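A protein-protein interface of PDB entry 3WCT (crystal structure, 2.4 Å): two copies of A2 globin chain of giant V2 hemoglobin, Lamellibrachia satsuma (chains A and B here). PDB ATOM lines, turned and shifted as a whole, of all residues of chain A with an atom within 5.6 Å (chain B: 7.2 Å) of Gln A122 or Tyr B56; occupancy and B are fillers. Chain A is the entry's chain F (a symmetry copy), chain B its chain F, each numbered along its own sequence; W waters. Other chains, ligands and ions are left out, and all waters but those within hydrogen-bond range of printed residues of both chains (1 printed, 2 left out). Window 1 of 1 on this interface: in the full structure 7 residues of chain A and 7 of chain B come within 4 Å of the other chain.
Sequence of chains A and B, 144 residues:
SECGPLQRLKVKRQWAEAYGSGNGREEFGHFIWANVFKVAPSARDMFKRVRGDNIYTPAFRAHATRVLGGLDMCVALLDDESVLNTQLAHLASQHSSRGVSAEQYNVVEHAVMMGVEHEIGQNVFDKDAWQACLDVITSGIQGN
The side-chain carboxylate (OE1) of Glu B26 is in hydrogen-bond range of the side-chain amide nitrogen (NE2) of Gln A122 (3.3 Å).
O of Asp B53 lies within hydrogen-bond range of NZ of Lys A127, 2.9 Å away.
OE1 of Glu A117 lies within hydrogen-bond range of OH of Tyr B56 (2.6 Å).
NH2 of Arg B61 is in hydrogen-bond range of OE1 of Gln A122, 2.9 Å away.
No position is printed for both chains.
Of the 11 pairs that touch across the chains among the printed residues, none has its exchanged pair printed and touching as well.
Of the printed residues of chain B, Met A114 touches Tyr B56.
Printed residues of chain B within 4 Å of Glu A117: Tyr B56.
Ile A120 touches none of the printed residues of chain B.
Of chain B, only Glu B26 (3.3 Å), His B30 (3.6 Å), Tyr B56 (3.5 Å) and Arg B61 (2.9 Å) come within 4 Å of Gln A122.
Tyr B56 touches just these residues of chain A: Met A114, Glu A117, Gln A122, Phe A125 and Lys A127.
Ala B59 touches none of the printed residues of chain A.
The nearest residue of chain B that does not touch Gln A122 is Glu B27 (4.2 Å).
The nearest printed residue of chain A that does not touch Asn B54 is Phe A125 (6.0 Å).
Printed residues of chain A that touch a printed residue of chain B: Met A114, Glu A117, Gln A122, Asn A123, Phe A125 and Lys A127.
Hydrophobic or aromatic side chains of chain A that line the printed part of chain B: Met A114 and Phe A125.
Of the 16 printed residues of chain B, 6 touch a printed residue of chain A.
Hydrophobic or aromatic side chains of chain B within 4 Å of the printed part of chain A: His B30 and Tyr B56.
Among the printed residues, no Asp or Glu carboxylate lies within 4 Å of a Lys or Arg side-chain nitrogen of the other chain.
The guanidinium group (NH2) of Arg B61 is in salt-bridge range of the side-chain carboxylate (OE2) of Glu B26.
The guanidinium group (NE) of Arg B51 lies within salt-bridge range of the side-chain carboxylate (OD1) of Asp B53 (2.9 Å).
The side-chain amide oxygen (OD1) of Asn B54 lies within hydrogen-bond range of the backbone NH (N) of Tyr B56.
The backbone carbonyl oxygen (O) of Asn B54 sits at hydrogen-bond distance from the side-chain hydroxyl (OG1) of Thr B57.
The guanidinium group (NE) of Arg B61 sits at hydrogen-bond distance from the backbone carbonyl oxygen (O) of Tyr B56 (2.9 Å).
Water W1 bridges OE1 of Glu A117 (2.5 Å) and OH of Tyr B56 (3.3 Å).
Among the printed residues, merely in contact across the chains: Asn A123 with Glu B26 (3.2 Å), Gln A122 with Tyr B56 (3.5 Å), Met A114 with Tyr B56 (3.6 Å), Gln A122 with His B30 (3.6 Å), Lys A127 with Asn B54 (3.6 Å), Phe A125 with Tyr B56 (3.7 Å) and Lys A127 with Tyr B56 (3.7 Å).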
ATOM      1  N   MET A 114     -20.507  -5.663   4.181  1.00  0.00           N
ATOM      2  CA  MET A 114     -20.243  -6.869   4.961  1.00  0.00           C
ATOM      3  C   MET A 114     -20.871  -8.056   4.266  1.00  0.00           C
ATOM      4  O   MET A 114     -20.253  -9.106   4.129  1.00  0.00           O
ATOM      5  CB  MET A 114     -20.804  -6.748   6.374  1.00  0.00           C
ATOM      6  CG  MET A 114     -20.031  -5.781   7.253  1.00  0.00           C
ATOM      7  SD  MET A 114     -18.285  -6.243   7.467  1.00  0.00           S
ATOM      8  CE  MET A 114     -17.514  -5.181   6.260  1.00  0.00           C
ATOM      9  N   GLU A 117     -18.814  -9.002   1.138  1.00  0.00           N
ATOM     10  CA  GLU A 117     -17.574  -9.620   1.590  1.00  0.00           C
ATOM     11  C   GLU A 117     -17.876 -11.040   2.076  1.00  0.00           C
ATOM     12  O   GLU A 117     -17.185 -11.999   1.721  1.00  0.00           O
ATOM     13  CB  GLU A 117     -16.979  -8.776   2.723  1.00  0.00           C
ATOM     14  CG  GLU A 117     -15.614  -9.208   3.176  1.00  0.00           C
ATOM     15  CD  GLU A 117     -15.633  -9.786   4.566  1.00  0.00           C
ATOM     16  OE1 GLU A 117     -15.532  -9.028   5.548  1.00  0.00           O
ATOM     17  OE2 GLU A 117     -15.768 -11.013   4.671  1.00  0.00           O
ATOM     18  N   ILE A 120     -18.448 -13.085  -1.050  1.00  0.00           N
ATOM     19  CA  ILE A 120     -17.329 -13.434  -1.910  1.00  0.00           C
ATOM     20  C   ILE A 120     -15.994 -13.678  -1.223  1.00  0.00           C
ATOM     21  O   ILE A 120     -15.062 -14.153  -1.850  1.00  0.00           O
ATOM     22  CB  ILE A 120     -17.155 -12.391  -3.041  1.00  0.00           C
ATOM     23  CG1 ILE A 120     -16.644 -11.068  -2.476  1.00  0.00           C
ATOM     24  CG2 ILE A 120     -18.493 -12.192  -3.751  1.00  0.00           C
ATOM     25  CD1 ILE A 120     -16.410 -10.011  -3.540  1.00  0.00           C
ATOM     26  N   GLY A 121     -15.897 -13.364   0.061  1.00  0.00           N
ATOM     27  CA  GLY A 121     -14.647 -13.617   0.765  1.00  0.00           C
ATOM     28  C   GLY A 121     -13.777 -12.413   1.033  1.00  0.00           C
ATOM     29  O   GLY A 121     -13.517 -11.608   0.142  1.00  0.00           O
ATOM     30  N   GLN A 122     -13.309 -12.308   2.270  1.00  0.00           N
ATOM     31  CA  GLN A 122     -12.459 -11.209   2.676  1.00  0.00           C
ATOM     32  C   GLN A 122     -11.182 -11.066   1.853  1.00  0.00           C
ATOM     33  O   GLN A 122     -10.670  -9.963   1.699  1.00  0.00           O
ATOM     34  CB  GLN A 122     -12.124 -11.323   4.171  1.00  0.00           C
ATOM     35  CG  GLN A 122     -11.266 -12.505   4.585  1.00  0.00           C
ATOM     36  CD  GLN A 122      -9.822 -12.359   4.152  1.00  0.00           C
ATOM     37  OE1 GLN A 122      -9.262 -11.261   4.175  1.00  0.00           O
ATOM     38  NE2 GLN A 122      -9.206 -13.467   3.763  1.00  0.00           N
ATOM     39  N   ASN A 123     -10.678 -12.161   1.300  1.00  0.00           N
ATOM     40  CA  ASN A 123      -9.442 -12.100   0.529  1.00  0.00           C
ATOM     41  C   ASN A 123      -9.547 -11.424  -0.841  1.00  0.00           C
ATOM     42  O   ASN A 123      -8.533 -11.094  -1.447  1.00  0.00           O
ATOM     43  CB  ASN A 123      -8.838 -13.508   0.390  1.00  0.00           C
ATOM     44  CG  ASN A 123      -9.567 -14.375  -0.623  1.00  0.00           C
ATOM     45  OD1 ASN A 123     -10.759 -14.665  -0.479  1.00  0.00           O
ATOM     46  ND2 ASN A 123      -8.847 -14.798  -1.659  1.00  0.00           N
ATOM     47  N   VAL A 124     -10.767 -11.204  -1.330  1.00  0.00           N
ATOM     48  CA  VAL A 124     -10.943 -10.553  -2.626  1.00  0.00           C
ATOM     49  C   VAL A 124     -11.734  -9.256  -2.514  1.00  0.00           C
ATOM     50  O   VAL A 124     -11.700  -8.419  -3.411  1.00  0.00           O
ATOM     51  CB  VAL A 124     -11.662 -11.481  -3.641  1.00  0.00           C
ATOM     52  CG1 VAL A 124     -10.821 -12.719  -3.909  1.00  0.00           C
ATOM     53  CG2 VAL A 124     -13.042 -11.866  -3.117  1.00  0.00           C
ATOM     54  N   PHE A 125     -12.448  -9.084  -1.409  1.00  0.00           N
ATOM     55  CA  PHE A 125     -13.257  -7.887  -1.218  1.00  0.00           C
ATOM     56  C   PHE A 125     -12.442  -6.609  -1.389  1.00  0.00           C
ATOM     57  O   PHE A 125     -11.432  -6.406  -0.701  1.00  0.00           O
ATOM     58  CB  PHE A 125     -13.901  -7.888   0.168  1.00  0.00           C
ATOM     59  CG  PHE A 125     -14.810  -6.726   0.404  1.00  0.00           C
ATOM     60  CD1 PHE A 125     -15.926  -6.519  -0.417  1.00  0.00           C
ATOM     61  CD2 PHE A 125     -14.546  -5.810   1.413  1.00  0.00           C
ATOM     62  CE1 PHE A 125     -16.766  -5.411  -0.236  1.00  0.00           C
ATOM     63  CE2 PHE A 125     -15.383  -4.694   1.600  1.00  0.00           C
ATOM     64  CZ  PHE A 125     -16.494  -4.498   0.770  1.00  0.00           C
ATOM     65  N   LYS A 127     -12.535  -3.105  -0.593  1.00  0.00           N
ATOM     66  CA  LYS A 127     -13.219  -2.076   0.173  1.00  0.00           C
ATOM     67  C   LYS A 127     -13.107  -0.642  -0.336  1.00  0.00           C
ATOM     68  O   LYS A 127     -14.087   0.103  -0.276  1.00  0.00           O
ATOM     69  CB  LYS A 127     -12.795  -2.106   1.644  1.00  0.00           C
ATOM     70  CG  LYS A 127     -13.648  -1.174   2.477  1.00  0.00           C
ATOM     71  CD  LYS A 127     -13.261  -1.138   3.916  1.00  0.00           C
ATOM     72  CE  LYS A 127     -14.114  -0.100   4.631  1.00  0.00           C
ATOM     73  NZ  LYS A 127     -13.578   0.241   5.974  1.00  0.00           N
ATOM     74  N   GLU B  26      -3.491 -15.391   6.704  1.00  0.00           N
ATOM     75  CA  GLU B  26      -4.164 -14.182   6.229  1.00  0.00           C
ATOM     76  C   GLU B  26      -5.540 -14.088   6.873  1.00  0.00           C
ATOM     77  O   GLU B  26      -5.871 -13.087   7.495  1.00  0.00           O
ATOM     78  CB  GLU B  26      -4.318 -14.178   4.705  1.00  0.00           C
ATOM     79  CG  GLU B  26      -4.966 -12.869   4.187  1.00  0.00           C
ATOM     80  CD  GLU B  26      -5.239 -12.863   2.687  1.00  0.00           C
ATOM     81  OE1 GLU B  26      -6.253 -13.448   2.251  1.00  0.00           O
ATOM     82  OE2 GLU B  26      -4.431 -12.278   1.937  1.00  0.00           O
ATOM     83  N   GLU B  27      -6.324 -15.152   6.731  1.00  0.00           N
ATOM     84  CA  GLU B  27      -7.664 -15.206   7.294  1.00  0.00           C
ATOM     85  C   GLU B  27      -7.633 -15.122   8.814  1.00  0.00           C
ATOM     86  O   GLU B  27      -8.524 -14.535   9.428  1.00  0.00           O
ATOM     87  CB  GLU B  27      -8.376 -16.487   6.858  1.00  0.00           C
ATOM     88  CG  GLU B  27      -9.831 -16.570   7.344  1.00  0.00           C
ATOM     89  CD  GLU B  27      -9.964 -17.034   8.802  1.00  0.00           C
ATOM     90  OE1 GLU B  27     -11.023 -16.770   9.407  1.00  0.00           O
ATOM     91  OE2 GLU B  27      -9.023 -17.673   9.339  1.00  0.00           O
ATOM     92  N   PHE B  28      -6.603 -15.702   9.416  1.00  0.00           N
ATOM     93  CA  PHE B  28      -6.474 -15.677  10.856  1.00  0.00           C
ATOM     94  C   PHE B  28      -6.337 -14.226  11.319  1.00  0.00           C
ATOM     95  O   PHE B  28      -7.118 -13.747  12.153  1.00  0.00           O
ATOM     96  CB  PHE B  28      -5.245 -16.476  11.265  1.00  0.00           C
ATOM     97  CG  PHE B  28      -5.072 -16.624  12.750  1.00  0.00           C
ATOM     98  CD1 PHE B  28      -3.796 -16.613  13.314  1.00  0.00           C
ATOM     99  CD2 PHE B  28      -6.179 -16.803  13.587  1.00  0.00           C
ATOM    100  CE1 PHE B  28      -3.621 -16.779  14.687  1.00  0.00           C
ATOM    101  CE2 PHE B  28      -6.012 -16.969  14.964  1.00  0.00           C
ATOM    102  CZ  PHE B  28      -4.727 -16.956  15.514  1.00  0.00           C
ATOM    103  N   HIS B  30      -6.982 -11.430   9.736  1.00  0.00           N
ATOM    104  CA  HIS B  30      -8.142 -10.614   9.397  1.00  0.00           C
ATOM    105  C   HIS B  30      -9.278 -10.762  10.419  1.00  0.00           C
ATOM    106  O   HIS B  30      -9.927  -9.783  10.776  1.00  0.00           O
ATOM    107  CB  HIS B  30      -8.645 -10.967   7.991  1.00  0.00           C
ATOM    108  CG  HIS B  30      -9.847 -10.187   7.584  1.00  0.00           C
ATOM    109  ND1 HIS B  30     -11.121 -10.529   7.984  1.00  0.00           N
ATOM    110  CD2 HIS B  30      -9.965  -9.032   6.888  1.00  0.00           C
ATOM    111  CE1 HIS B  30     -11.972  -9.618   7.552  1.00  0.00           C
ATOM    112  NE2 HIS B  30     -11.297  -8.698   6.886  1.00  0.00           N
ATOM    113  N   PHE B  31      -9.511 -11.980  10.899  1.00  0.00           N
ATOM    114  CA  PHE B  31     -10.566 -12.225  11.886  1.00  0.00           C
ATOM    115  C   PHE B  31     -10.253 -11.488  13.184  1.00  0.00           C
ATOM    116  O   PHE B  31     -11.137 -10.905  13.800  1.00  0.00           O
ATOM    117  CB  PHE B  31     -10.685 -13.722  12.178  1.00  0.00           C
ATOM    118  CG  PHE B  31     -11.859 -14.093  13.065  1.00  0.00           C
ATOM    119  CD1 PHE B  31     -13.092 -14.439  12.512  1.00  0.00           C
ATOM    120  CD2 PHE B  31     -11.718 -14.141  14.447  1.00  0.00           C
ATOM    121  CE1 PHE B  31     -14.161 -14.839  13.335  1.00  0.00           C
ATOM    122  CE2 PHE B  31     -12.777 -14.534  15.270  1.00  0.00           C
ATOM    123  CZ  PHE B  31     -13.993 -14.883  14.719  1.00  0.00           C
ATOM    124  N   ALA B  34     -10.567  -7.633  12.529  1.00  0.00           N
ATOM    125  CA  ALA B  34     -11.936  -7.213  12.253  1.00  0.00           C
ATOM    126  C   ALA B  34     -12.598  -7.118  13.621  1.00  0.00           C
ATOM    127  O   ALA B  34     -13.396  -6.226  13.881  1.00  0.00           O
ATOM    128  CB  ALA B  34     -12.664  -8.245  11.401  1.00  0.00           C
ATOM    129  N   ARG B  51      -2.979   1.979   6.720  1.00  0.00           N
ATOM    130  CA  ARG B  51      -4.364   1.829   6.290  1.00  0.00           C
ATOM    131  C   ARG B  51      -5.252   1.086   7.289  1.00  0.00           C
ATOM    132  O   ARG B  51      -5.973   0.149   6.927  1.00  0.00           O
ATOM    133  CB  ARG B  51      -4.400   1.133   4.933  1.00  0.00           C
ATOM    134  CG  ARG B  51      -3.787   1.969   3.829  1.00  0.00           C
ATOM    135  CD  ARG B  51      -4.446   3.349   3.768  1.00  0.00           C
ATOM    136  NE  ARG B  51      -5.893   3.257   3.598  1.00  0.00           N
ATOM    137  CZ  ARG B  51      -6.482   2.845   2.484  1.00  0.00           C
ATOM    138  NH1 ARG B  51      -5.742   2.498   1.436  1.00  0.00           N
ATOM    139  NH2 ARG B  51      -7.809   2.759   2.425  1.00  0.00           N
ATOM    140  N   ASP B  53      -7.817   1.899   8.318  1.00  0.00           N
ATOM    141  CA  ASP B  53      -9.200   2.220   7.983  1.00  0.00           C
ATOM    142  C   ASP B  53      -9.726   1.146   7.036  1.00  0.00           C
ATOM    143  O   ASP B  53     -10.934   0.926   6.923  1.00  0.00           O
ATOM    144  CB  ASP B  53      -9.267   3.582   7.280  1.00  0.00           C
ATOM    145  CG  ASP B  53      -8.421   3.626   6.027  1.00  0.00           C
ATOM    146  OD1 ASP B  53      -7.189   3.467   6.130  1.00  0.00           O
ATOM    147  OD2 ASP B  53      -8.984   3.806   4.932  1.00  0.00           O
ATOM    148  N   ASN B  54      -8.801   0.476   6.358  1.00  0.00           N
ATOM    149  CA  ASN B  54      -9.152  -0.562   5.394  1.00  0.00           C
ATOM    150  C   ASN B  54      -8.259  -1.788   5.569  1.00  0.00           C
ATOM    151  O   ASN B  54      -7.235  -1.919   4.886  1.00  0.00           O
ATOM    152  CB  ASN B  54      -8.997  -0.003   3.976  1.00  0.00           C
ATOM    153  CG  ASN B  54      -9.379  -1.001   2.908  1.00  0.00           C
ATOM    154  OD1 ASN B  54      -9.542  -2.186   3.183  1.00  0.00           O
ATOM    155  ND2 ASN B  54      -9.518  -0.524   1.675  1.00  0.00           N
ATOM    156  N   ILE B  55      -8.662  -2.688   6.469  1.00  0.00           N
ATOM    157  CA  ILE B  55      -7.896  -3.906   6.753  1.00  0.00           C
ATOM    158  C   ILE B  55      -7.785  -4.866   5.585  1.00  0.00           C
ATOM    159  O   ILE B  55      -7.069  -5.853   5.661  1.00  0.00           O
ATOM    160  CB  ILE B  55      -8.473  -4.703   7.958  1.00  0.00           C
ATOM    161  CG1 ILE B  55      -9.840  -5.293   7.605  1.00  0.00           C
ATOM    162  CG2 ILE B  55      -8.586  -3.789   9.182  1.00  0.00           C
ATOM    163  CD1 ILE B  55     -10.437  -6.155   8.724  1.00  0.00           C
ATOM    164  N   TYR B  56      -8.484  -4.588   4.499  1.00  0.00           N
ATOM    165  CA  TYR B  56      -8.400  -5.470   3.346  1.00  0.00           C
ATOM    166  C   TYR B  56      -7.167  -5.163   2.483  1.00  0.00           C
ATOM    167  O   TYR B  56      -6.806  -5.931   1.603  1.00  0.00           O
ATOM    168  CB  TYR B  56      -9.683  -5.358   2.517  1.00  0.00           C
ATOM    169  CG  TYR B  56     -10.931  -5.710   3.300  1.00  0.00           C
ATOM    170  CD1 TYR B  56     -11.381  -7.026   3.390  1.00  0.00           C
ATOM    171  CD2 TYR B  56     -11.657  -4.726   3.969  1.00  0.00           C
ATOM    172  CE1 TYR B  56     -12.526  -7.354   4.125  1.00  0.00           C
ATOM    173  CE2 TYR B  56     -12.798  -5.042   4.708  1.00  0.00           C
ATOM    174  CZ  TYR B  56     -13.228  -6.356   4.778  1.00  0.00           C
ATOM    175  OH  TYR B  56     -14.379  -6.652   5.476  1.00  0.00           O
ATOM    176  N   THR B  57      -6.498  -4.054   2.754  1.00  0.00           N
ATOM    177  CA  THR B  57      -5.324  -3.698   1.956  1.00  0.00           C
ATOM    178  C   THR B  57      -4.046  -4.446   2.319  1.00  0.00           C
ATOM    179  O   THR B  57      -3.889  -4.950   3.435  1.00  0.00           O
ATOM    180  CB  THR B  57      -4.965  -2.210   2.078  1.00  0.00           C
ATOM    181  OG1 THR B  57      -4.703  -1.918   3.452  1.00  0.00           O
ATOM    182  CG2 THR B  57      -6.088  -1.324   1.561  1.00  0.00           C
ATOM    183  N   PRO B  58      -3.113  -4.521   1.362  1.00  0.00           N
ATOM    184  CA  PRO B  58      -1.827  -5.185   1.549  1.00  0.00           C
ATOM    185  C   PRO B  58      -1.029  -4.500   2.673  1.00  0.00           C
ATOM    186  O   PRO B  58      -0.285  -5.149   3.417  1.00  0.00           O
ATOM    187  CB  PRO B  58      -1.164  -5.019   0.190  1.00  0.00           C
ATOM    188  CG  PRO B  58      -2.332  -5.144  -0.747  1.00  0.00           C
ATOM    189  CD  PRO B  58      -3.388  -4.298  -0.070  1.00  0.00           C
ATOM    190  N   ALA B  59      -1.191  -3.190   2.802  1.00  0.00           N
ATOM    191  CA  ALA B  59      -0.484  -2.455   3.835  1.00  0.00           C
ATOM    192  C   ALA B  59      -0.956  -2.919   5.208  1.00  0.00           C
ATOM    193  O   ALA B  59      -0.148  -3.240   6.073  1.00  0.00           O
ATOM    194  CB  ALA B  59      -0.710  -0.950   3.668  1.00  0.00           C
ATOM    195  N   PHE B  60      -2.263  -2.976   5.415  1.00  0.00           N
ATOM    196  CA  PHE B  60      -2.725  -3.416   6.717  1.00  0.00           C
ATOM    197  C   PHE B  60      -2.427  -4.894   6.936  1.00  0.00           C
ATOM    198  O   PHE B  60      -2.070  -5.312   8.035  1.00  0.00           O
ATOM    199  CB  PHE B  60      -4.220  -3.198   6.920  1.00  0.00           C
ATOM    200  CG  PHE B  60      -4.643  -3.464   8.322  1.00  0.00           C
ATOM    201  CD1 PHE B  60      -4.546  -2.468   9.283  1.00  0.00           C
ATOM    202  CD2 PHE B  60      -5.037  -4.747   8.712  1.00  0.00           C
ATOM    203  CE1 PHE B  60      -4.827  -2.735  10.607  1.00  0.00           C
ATOM    204  CE2 PHE B  60      -5.320  -5.024  10.031  1.00  0.00           C
ATOM    205  CZ  PHE B  60      -5.217  -4.020  10.989  1.00  0.00           C
ATOM    206  N   ARG B  61      -2.581  -5.692   5.895  1.00  0.00           N
ATOM    207  CA  ARG B  61      -2.307  -7.104   6.043  1.00  0.00           C
ATOM    208  C   ARG B  61      -0.845  -7.310   6.438  1.00  0.00           C
ATOM    209  O   ARG B  61      -0.517  -8.250   7.164  1.00  0.00           O
ATOM    210  CB  ARG B  61      -2.628  -7.837   4.741  1.00  0.00           C
ATOM    211  CG  ARG B  61      -4.133  -7.865   4.401  1.00  0.00           C
ATOM    212  CD  ARG B  61      -4.343  -8.617   3.094  1.00  0.00           C
ATOM    213  NE  ARG B  61      -5.689  -8.490   2.552  1.00  0.00           N
ATOM    214  CZ  ARG B  61      -6.759  -9.116   3.027  1.00  0.00           C
ATOM    215  NH1 ARG B  61      -7.940  -8.928   2.452  1.00  0.00           N
ATOM    216  NH2 ARG B  61      -6.651  -9.929   4.069  1.00  0.00           N
HETATM  217  O   HOH W   1     -14.725  -8.940   7.889  1.00  0.00           O
